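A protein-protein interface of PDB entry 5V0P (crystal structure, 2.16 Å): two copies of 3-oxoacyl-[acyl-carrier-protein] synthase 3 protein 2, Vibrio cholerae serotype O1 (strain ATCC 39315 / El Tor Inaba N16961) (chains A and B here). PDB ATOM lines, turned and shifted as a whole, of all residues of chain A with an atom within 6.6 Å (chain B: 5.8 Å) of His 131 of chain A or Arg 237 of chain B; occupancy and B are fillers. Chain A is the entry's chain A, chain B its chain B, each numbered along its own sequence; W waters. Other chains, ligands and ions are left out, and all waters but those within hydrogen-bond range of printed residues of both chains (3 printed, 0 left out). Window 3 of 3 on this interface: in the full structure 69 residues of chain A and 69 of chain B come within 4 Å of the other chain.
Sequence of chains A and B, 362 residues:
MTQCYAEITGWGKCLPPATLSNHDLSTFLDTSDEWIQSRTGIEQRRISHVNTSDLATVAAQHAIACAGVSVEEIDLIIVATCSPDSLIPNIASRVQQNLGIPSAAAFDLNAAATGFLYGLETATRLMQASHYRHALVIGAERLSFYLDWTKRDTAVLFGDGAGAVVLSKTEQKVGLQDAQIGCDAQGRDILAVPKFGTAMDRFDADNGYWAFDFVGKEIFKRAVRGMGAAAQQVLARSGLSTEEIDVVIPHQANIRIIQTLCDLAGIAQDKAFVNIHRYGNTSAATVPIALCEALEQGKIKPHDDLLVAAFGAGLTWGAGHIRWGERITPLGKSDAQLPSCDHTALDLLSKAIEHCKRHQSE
His 131 of chain A touches four residues of chain B.
Arg 237 of chain B touches one residue of chain A.
Of the printed residues of chain A, Ala 179 of chain B touches His 131.
Of the printed residues of chain A, Asp 178 of chain B touches His 131 (2.7 Å).
Printed residues of chain A within 4 Å of Gln 180 of chain B: His 131 (3.4 Å).
Printed residues of chain B within 4 Å of Tyr 132 of chain A: Glu 121.
Of the printed residues of chain A, Glu 121 of chain B touches Leu 126 and Tyr 132.
Ser 130 of chain A touches none of the printed residues of chain B.
Ala 129 of chain A touches none of the printed residues of chain B.
The nearest printed residue of chain A that does not touch Arg 237 of chain B is Ser 130 of chain A (6.7 Å).
Among the printed residues, merely in contact across the chains: His 131 of chain A with Gln 180 of chain B (3.4 Å), His 131 of chain A with Arg 237 of chain B (3.5 Å) and Leu 126 of chain A with Glu 121 of chain B (3.9 Å).
Hydrophobic or aromatic side chains of chain A within 4 Å of the printed part of chain B: Leu 126, His 131 and Tyr 132.
Of the 12 printed residues of chain B, 5 touch a printed residue of chain A.
Along chain B the printed residues that touch a printed residue of chain A span positions 121 to 237.
Among the printed residues, no Asp or Glu carboxylate lies within 4 Å of a Lys or Arg side-chain nitrogen of the other chain.
No position is printed for both chains.
Of the 6 pairs that touch across the chains among the printed residues, none has its exchanged pair printed and touching as well.
Water W3 lies within hydrogen-bond range of the side-chain hydroxyl (OG) of Ser 130 of chain A, the side-chain carboxylate (OE2) of Glu 121 of chain B, the backbone carbonyl oxygen (O) of Ala 179 of chain B and a ring nitrogen (NE2) of His 131 of chain A.
Water W1 lies within hydrogen-bond range of the side-chain carboxylate (OD2) of Asp 178 of chain B, the side-chain amide oxygen (OE1) of Gln 180 of chain B, the guanidinium group (NE) of Arg 237 of chain B and a ring nitrogen (NE2) of His 131 of chain A.
Water W2 bridges the side-chain amide nitrogen (NE2) of Gln 180 of chain B (2.8 Å) and the backbone carbonyl oxygen (O) of His 131 of chain A (3.1 Å).
NE2 of His 131 of chain A is in hydrogen-bond range of OD1 of Asp 178 of chain B, at 2.7 Å.
A ring nitrogen (NE2) of His 131 of chain A sits close to the backbone carbonyl oxygen of Ala 179 of chain B (3.3 Å).
The side-chain carboxylate (OE2) of Glu 121 of chain B is in hydrogen-bond range of the side-chain hydroxyl (OH) of Tyr 132 of chain A (2.7 Å).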
ATOM      1  N   ASP A  75      -6.836   5.065 -15.863  1.00  0.00           N
ATOM      2  CA  ASP A  75      -7.213   6.435 -16.280  1.00  0.00           C
ATOM      3  C   ASP A  75      -8.398   6.481 -17.241  1.00  0.00           C
ATOM      4  O   ASP A  75      -8.912   7.552 -17.516  1.00  0.00           O
ATOM      5  CB  ASP A  75      -6.015   7.101 -16.956  1.00  0.00           C
ATOM      6  CG  ASP A  75      -4.858   7.335 -16.003  1.00  0.00           C
ATOM      7  OD1 ASP A  75      -5.086   7.474 -14.779  1.00  0.00           O
ATOM      8  OD2 ASP A  75      -3.698   7.354 -16.490  1.00  0.00           O
ATOM      9  N   LEU A 126      -6.277   7.215 -27.757  1.00  0.00           N
ATOM     10  CA  LEU A 126      -6.305   8.111 -26.587  1.00  0.00           C
ATOM     11  C   LEU A 126      -4.981   8.072 -25.871  1.00  0.00           C
ATOM     12  O   LEU A 126      -4.390   9.117 -25.556  1.00  0.00           O
ATOM     13  CB  LEU A 126      -7.440   7.720 -25.632  1.00  0.00           C
ATOM     14  CG  LEU A 126      -8.848   8.131 -26.104  1.00  0.00           C
ATOM     15  CD1 LEU A 126      -9.922   7.394 -25.340  1.00  0.00           C
ATOM     16  CD2 LEU A 126      -9.047   9.632 -25.980  1.00  0.00           C
ATOM     17  N   MET A 127      -4.485   6.854 -25.641  1.00  0.00           N
ATOM     18  CA  MET A 127      -3.238   6.687 -24.900  1.00  0.00           C
ATOM     19  C   MET A 127      -2.043   7.170 -25.682  1.00  0.00           C
ATOM     20  O   MET A 127      -1.125   7.731 -25.100  1.00  0.00           O
ATOM     21  CB  MET A 127      -3.038   5.227 -24.466  1.00  0.00           C
ATOM     22  CG  MET A 127      -4.091   4.771 -23.461  1.00  0.00           C
ATOM     23  SD  MET A 127      -4.093   3.003 -23.167  1.00  0.00           S
ATOM     24  CE  MET A 127      -2.451   2.796 -22.485  1.00  0.00           C
ATOM     25  N   ALA A 129      -1.958   9.590 -28.036  1.00  0.00           N
ATOM     26  CA  ALA A 129      -2.046  11.037 -28.265  1.00  0.00           C
ATOM     27  C   ALA A 129      -2.173  11.878 -26.987  1.00  0.00           C
ATOM     28  O   ALA A 129      -1.945  13.079 -27.037  1.00  0.00           O
ATOM     29  CB  ALA A 129      -3.220  11.349 -29.216  1.00  0.00           C
ATOM     30  N   SER A 130      -2.549  11.271 -25.856  1.00  0.00           N
ATOM     31  CA  SER A 130      -2.735  12.037 -24.629  1.00  0.00           C
ATOM     32  C   SER A 130      -2.303  11.271 -23.373  1.00  0.00           C
ATOM     33  O   SER A 130      -1.564  10.287 -23.460  1.00  0.00           O
ATOM     34  CB  SER A 130      -4.170  12.546 -24.549  1.00  0.00           C
ATOM     35  OG  SER A 130      -4.192  13.701 -23.718  1.00  0.00           O
ATOM     36  N   HIS A 131      -2.740  11.744 -22.209  1.00  0.00           N
ATOM     37  CA  HIS A 131      -2.196  11.319 -20.895  1.00  0.00           C
ATOM     38  C   HIS A 131      -3.195  10.333 -20.240  1.00  0.00           C
ATOM     39  O   HIS A 131      -3.990  10.692 -19.332  1.00  0.00           O
ATOM     40  CB  HIS A 131      -1.932  12.547 -20.001  1.00  0.00           C
ATOM     41  CG  HIS A 131      -2.968  13.616 -20.134  1.00  0.00           C
ATOM     42  ND1 HIS A 131      -4.285  13.407 -19.788  1.00  0.00           N
ATOM     43  CD2 HIS A 131      -2.915  14.857 -20.685  1.00  0.00           C
ATOM     44  CE1 HIS A 131      -4.995  14.488 -20.080  1.00  0.00           C
ATOM     45  NE2 HIS A 131      -4.183  15.389 -20.613  1.00  0.00           N
ATOM     46  N   TYR A 132      -3.200   9.119 -20.774  1.00  0.00           N
ATOM     47  CA  TYR A 132      -3.878   7.984 -20.170  1.00  0.00           C
ATOM     48  C   TYR A 132      -2.772   6.924 -20.024  1.00  0.00           C
ATOM     49  O   TYR A 132      -2.196   6.490 -21.022  1.00  0.00           O
ATOM     50  CB  TYR A 132      -5.052   7.493 -21.037  1.00  0.00           C
ATOM     51  CG  TYR A 132      -6.084   8.554 -21.346  1.00  0.00           C
ATOM     52  CD1 TYR A 132      -7.169   8.785 -20.492  1.00  0.00           C
ATOM     53  CD2 TYR A 132      -5.970   9.350 -22.483  1.00  0.00           C
ATOM     54  CE1 TYR A 132      -8.100   9.780 -20.760  1.00  0.00           C
ATOM     55  CE2 TYR A 132      -6.909  10.335 -22.776  1.00  0.00           C
ATOM     56  CZ  TYR A 132      -7.969  10.550 -21.917  1.00  0.00           C
ATOM     57  OH  TYR A 132      -8.892  11.531 -22.184  1.00  0.00           O
ATOM     58  N   ARG A 133      -2.451   6.566 -18.780  1.00  0.00           N
ATOM     59  CA  ARG A 133      -1.356   5.630 -18.483  1.00  0.00           C
ATOM     60  C   ARG A 133      -1.790   4.181 -18.693  1.00  0.00           C
ATOM     61  O   ARG A 133      -1.030   3.378 -19.216  1.00  0.00           O
ATOM     62  CB  ARG A 133      -0.882   5.791 -17.032  1.00  0.00           C
ATOM     63  CG  ARG A 133      -0.324   7.172 -16.673  1.00  0.00           C
ATOM     64  CD  ARG A 133      -0.226   7.346 -15.148  1.00  0.00           C
ATOM     65  NE  ARG A 133      -1.557   7.408 -14.530  1.00  0.00           N
ATOM     66  CZ  ARG A 133      -1.810   7.450 -13.222  1.00  0.00           C
ATOM     67  NH1 ARG A 133      -0.824   7.455 -12.334  1.00  0.00           N
ATOM     68  NH2 ARG A 133      -3.069   7.509 -12.794  1.00  0.00           N
ATOM     69  N   LYS A 169       0.590   1.827 -21.178  1.00  0.00           N
ATOM     70  CA  LYS A 169       1.379   2.649 -22.066  1.00  0.00           C
ATOM     71  C   LYS A 169       2.832   2.202 -22.021  1.00  0.00           C
ATOM     72  O   LYS A 169       3.349   1.906 -20.949  1.00  0.00           O
ATOM     73  CB  LYS A 169       1.233   4.105 -21.665  1.00  0.00           C
ATOM     74  CG  LYS A 169       1.759   5.112 -22.666  1.00  0.00           C
ATOM     75  CD  LYS A 169       1.316   6.516 -22.261  1.00  0.00           C
ATOM     76  CE  LYS A 169       1.347   7.511 -23.395  1.00  0.00           C
ATOM     77  NZ  LYS A 169       0.415   8.637 -23.106  1.00  0.00           N
ATOM     78  N   GLU B 121     -12.866  14.911 -27.475  1.00  0.00           N
ATOM     79  CA  GLU B 121     -11.596  14.355 -27.035  1.00  0.00           C
ATOM     80  C   GLU B 121     -11.255  13.101 -27.832  1.00  0.00           C
ATOM     81  O   GLU B 121     -10.139  12.970 -28.339  1.00  0.00           O
ATOM     82  CB  GLU B 121     -11.636  14.047 -25.519  1.00  0.00           C
ATOM     83  CG  GLU B 121     -10.560  13.147 -24.936  1.00  0.00           C
ATOM     84  CD  GLU B 121      -9.178  13.747 -24.913  1.00  0.00           C
ATOM     85  OE1 GLU B 121      -8.900  14.807 -25.517  1.00  0.00           O
ATOM     86  OE2 GLU B 121      -8.319  13.120 -24.277  1.00  0.00           O
ATOM     87  N   ASP B 178      -5.202  20.646 -24.779  1.00  0.00           N
ATOM     88  CA  ASP B 178      -5.409  19.740 -23.652  1.00  0.00           C
ATOM     89  C   ASP B 178      -6.900  19.611 -23.249  1.00  0.00           C
ATOM     90  O   ASP B 178      -7.721  20.555 -23.401  1.00  0.00           O
ATOM     91  CB  ASP B 178      -4.547  20.137 -22.450  1.00  0.00           C
ATOM     92  CG  ASP B 178      -4.531  19.055 -21.367  1.00  0.00           C
ATOM     93  OD1 ASP B 178      -4.497  17.836 -21.692  1.00  0.00           O
ATOM     94  OD2 ASP B 178      -4.604  19.421 -20.183  1.00  0.00           O
ATOM     95  N   ALA B 179      -7.246  18.401 -22.815  1.00  0.00           N
ATOM     96  CA  ALA B 179      -8.512  18.103 -22.195  1.00  0.00           C
ATOM     97  C   ALA B 179      -8.274  17.199 -21.001  1.00  0.00           C
ATOM     98  O   ALA B 179      -7.313  16.436 -20.958  1.00  0.00           O
ATOM     99  CB  ALA B 179      -9.468  17.433 -23.159  1.00  0.00           C
ATOM    100  N   GLN B 180      -9.182  17.283 -20.048  1.00  0.00           N
ATOM    101  CA  GLN B 180      -9.159  16.416 -18.907  1.00  0.00           C
ATOM    102  C   GLN B 180     -10.562  15.938 -18.699  1.00  0.00           C
ATOM    103  O   GLN B 180     -11.431  16.710 -18.296  1.00  0.00           O
ATOM    104  CB  GLN B 180      -8.662  17.169 -17.670  1.00  0.00           C
ATOM    105  CG  GLN B 180      -8.386  16.245 -16.497  1.00  0.00           C
ATOM    106  CD  GLN B 180      -7.160  15.378 -16.723  1.00  0.00           C
ATOM    107  OE1 GLN B 180      -6.101  15.874 -17.128  1.00  0.00           O
ATOM    108  NE2 GLN B 180      -7.289  14.075 -16.435  1.00  0.00           N
ATOM    109  N   GLN B 232      -8.882  23.486 -13.957  1.00  0.00           N
ATOM    110  CA  GLN B 232      -7.556  23.801 -13.403  1.00  0.00           C
ATOM    111  C   GLN B 232      -6.406  22.973 -13.990  1.00  0.00           C
ATOM    112  O   GLN B 232      -5.355  23.526 -14.307  1.00  0.00           O
ATOM    113  CB  GLN B 232      -7.551  23.655 -11.873  1.00  0.00           C
ATOM    114  CG  GLN B 232      -8.353  24.698 -11.109  1.00  0.00           C
ATOM    115  CD  GLN B 232      -7.988  26.123 -11.492  1.00  0.00           C
ATOM    116  OE1 GLN B 232      -8.852  26.905 -11.923  1.00  0.00           O
ATOM    117  NE2 GLN B 232      -6.711  26.456 -11.394  1.00  0.00           N
ATOM    118  N   GLN B 233      -6.608  21.668 -14.138  1.00  0.00           N
ATOM    119  CA  GLN B 233      -5.613  20.802 -14.772  1.00  0.00           C
ATOM    120  C   GLN B 233      -5.373  21.206 -16.215  1.00  0.00           C
ATOM    121  O   GLN B 233      -4.232  21.227 -16.655  1.00  0.00           O
ATOM    122  CB  GLN B 233      -6.008  19.303 -14.728  1.00  0.00           C
ATOM    123  CG  GLN B 233      -5.994  18.674 -13.338  1.00  0.00           C
ATOM    124  CD  GLN B 233      -4.675  18.860 -12.594  1.00  0.00           C
ATOM    125  OE1 GLN B 233      -3.614  18.652 -13.154  1.00  0.00           O
ATOM    126  NE2 GLN B 233      -4.750  19.255 -11.331  1.00  0.00           N
ATOM    127  N   VAL B 234      -6.438  21.532 -16.941  1.00  0.00           N
ATOM    128  CA  VAL B 234      -6.277  21.979 -18.328  1.00  0.00           C
ATOM    129  C   VAL B 234      -5.473  23.272 -18.377  1.00  0.00           C
ATOM    130  O   VAL B 234      -4.498  23.365 -19.140  1.00  0.00           O
ATOM    131  CB  VAL B 234      -7.628  22.139 -19.067  1.00  0.00           C
ATOM    132  CG1 VAL B 234      -7.465  22.889 -20.371  1.00  0.00           C
ATOM    133  CG2 VAL B 234      -8.233  20.773 -19.326  1.00  0.00           C
ATOM    134  N   LEU B 235      -5.858  24.270 -17.590  1.00  0.00           N
ATOM    135  CA  LEU B 235      -5.114  25.548 -17.613  1.00  0.00           C
ATOM    136  C   LEU B 235      -3.651  25.375 -17.152  1.00  0.00           C
ATOM    137  O   LEU B 235      -2.735  25.819 -17.826  1.00  0.00           O
ATOM    138  CB  LEU B 235      -5.816  26.602 -16.784  1.00  0.00           C
ATOM    139  CG  LEU B 235      -7.221  26.951 -17.264  1.00  0.00           C
ATOM    140  CD1 LEU B 235      -7.970  27.789 -16.244  1.00  0.00           C
ATOM    141  CD2 LEU B 235      -7.184  27.621 -18.615  1.00  0.00           C
ATOM    142  N   ALA B 236      -3.445  24.683 -16.042  1.00  0.00           N
ATOM    143  CA  ALA B 236      -2.096  24.437 -15.499  1.00  0.00           C
ATOM    144  C   ALA B 236      -1.161  23.749 -16.481  1.00  0.00           C
ATOM    145  O   ALA B 236      -0.067  24.223 -16.731  1.00  0.00           O
ATOM    146  CB  ALA B 236      -2.189  23.605 -14.217  1.00  0.00           C
ATOM    147  N   ARG B 237      -1.609  22.630 -17.038  1.00  0.00           N
ATOM    148  CA  ARG B 237      -0.813  21.853 -18.005  1.00  0.00           C
ATOM    149  C   ARG B 237      -0.481  22.635 -19.285  1.00  0.00           C
ATOM    150  O   ARG B 237       0.581  22.425 -19.886  1.00  0.00           O
ATOM    151  CB  ARG B 237      -1.544  20.544 -18.362  1.00  0.00           C
ATOM    152  CG  ARG B 237      -0.705  19.515 -19.126  1.00  0.00           C
ATOM    153  CD  ARG B 237      -1.494  18.263 -19.506  1.00  0.00           C
ATOM    154  NE  ARG B 237      -1.493  17.238 -18.457  1.00  0.00           N
ATOM    155  CZ  ARG B 237      -0.671  16.185 -18.380  1.00  0.00           C
ATOM    156  NH1 ARG B 237      -0.801  15.330 -17.361  1.00  0.00           N
ATOM    157  NH2 ARG B 237       0.275  15.957 -19.296  1.00  0.00           N
ATOM    158  N   SER B 238      -1.376  23.538 -19.686  1.00  0.00           N
ATOM    159  CA  SER B 238      -1.236  24.290 -20.924  1.00  0.00           C
ATOM    160  C   SER B 238      -0.445  25.613 -20.795  1.00  0.00           C
ATOM    161  O   SER B 238      -0.233  26.300 -21.790  1.00  0.00           O
ATOM    162  CB  SER B 238      -2.628  24.580 -21.462  1.00  0.00           C
ATOM    163  OG  SER B 238      -3.314  25.377 -20.539  1.00  0.00           O
ATOM    164  N   GLY B 239      -0.062  25.988 -19.572  1.00  0.00           N
ATOM    165  CA  GLY B 239       0.681  27.233 -19.324  1.00  0.00           C
ATOM    166  C   GLY B 239      -0.127  28.507 -19.531  1.00  0.00           C
ATOM    167  O   GLY B 239       0.443  29.585 -19.659  1.00  0.00           O
HETATM  168  O   HOH W   1      -4.436  17.655 -18.216  1.00  0.00           O
HETATM  169  O   HOH W   2      -6.628  11.928 -18.162  1.00  0.00           O
HETATM  170  O   HOH W   3      -6.528  14.607 -23.071  1.00  0.00           O
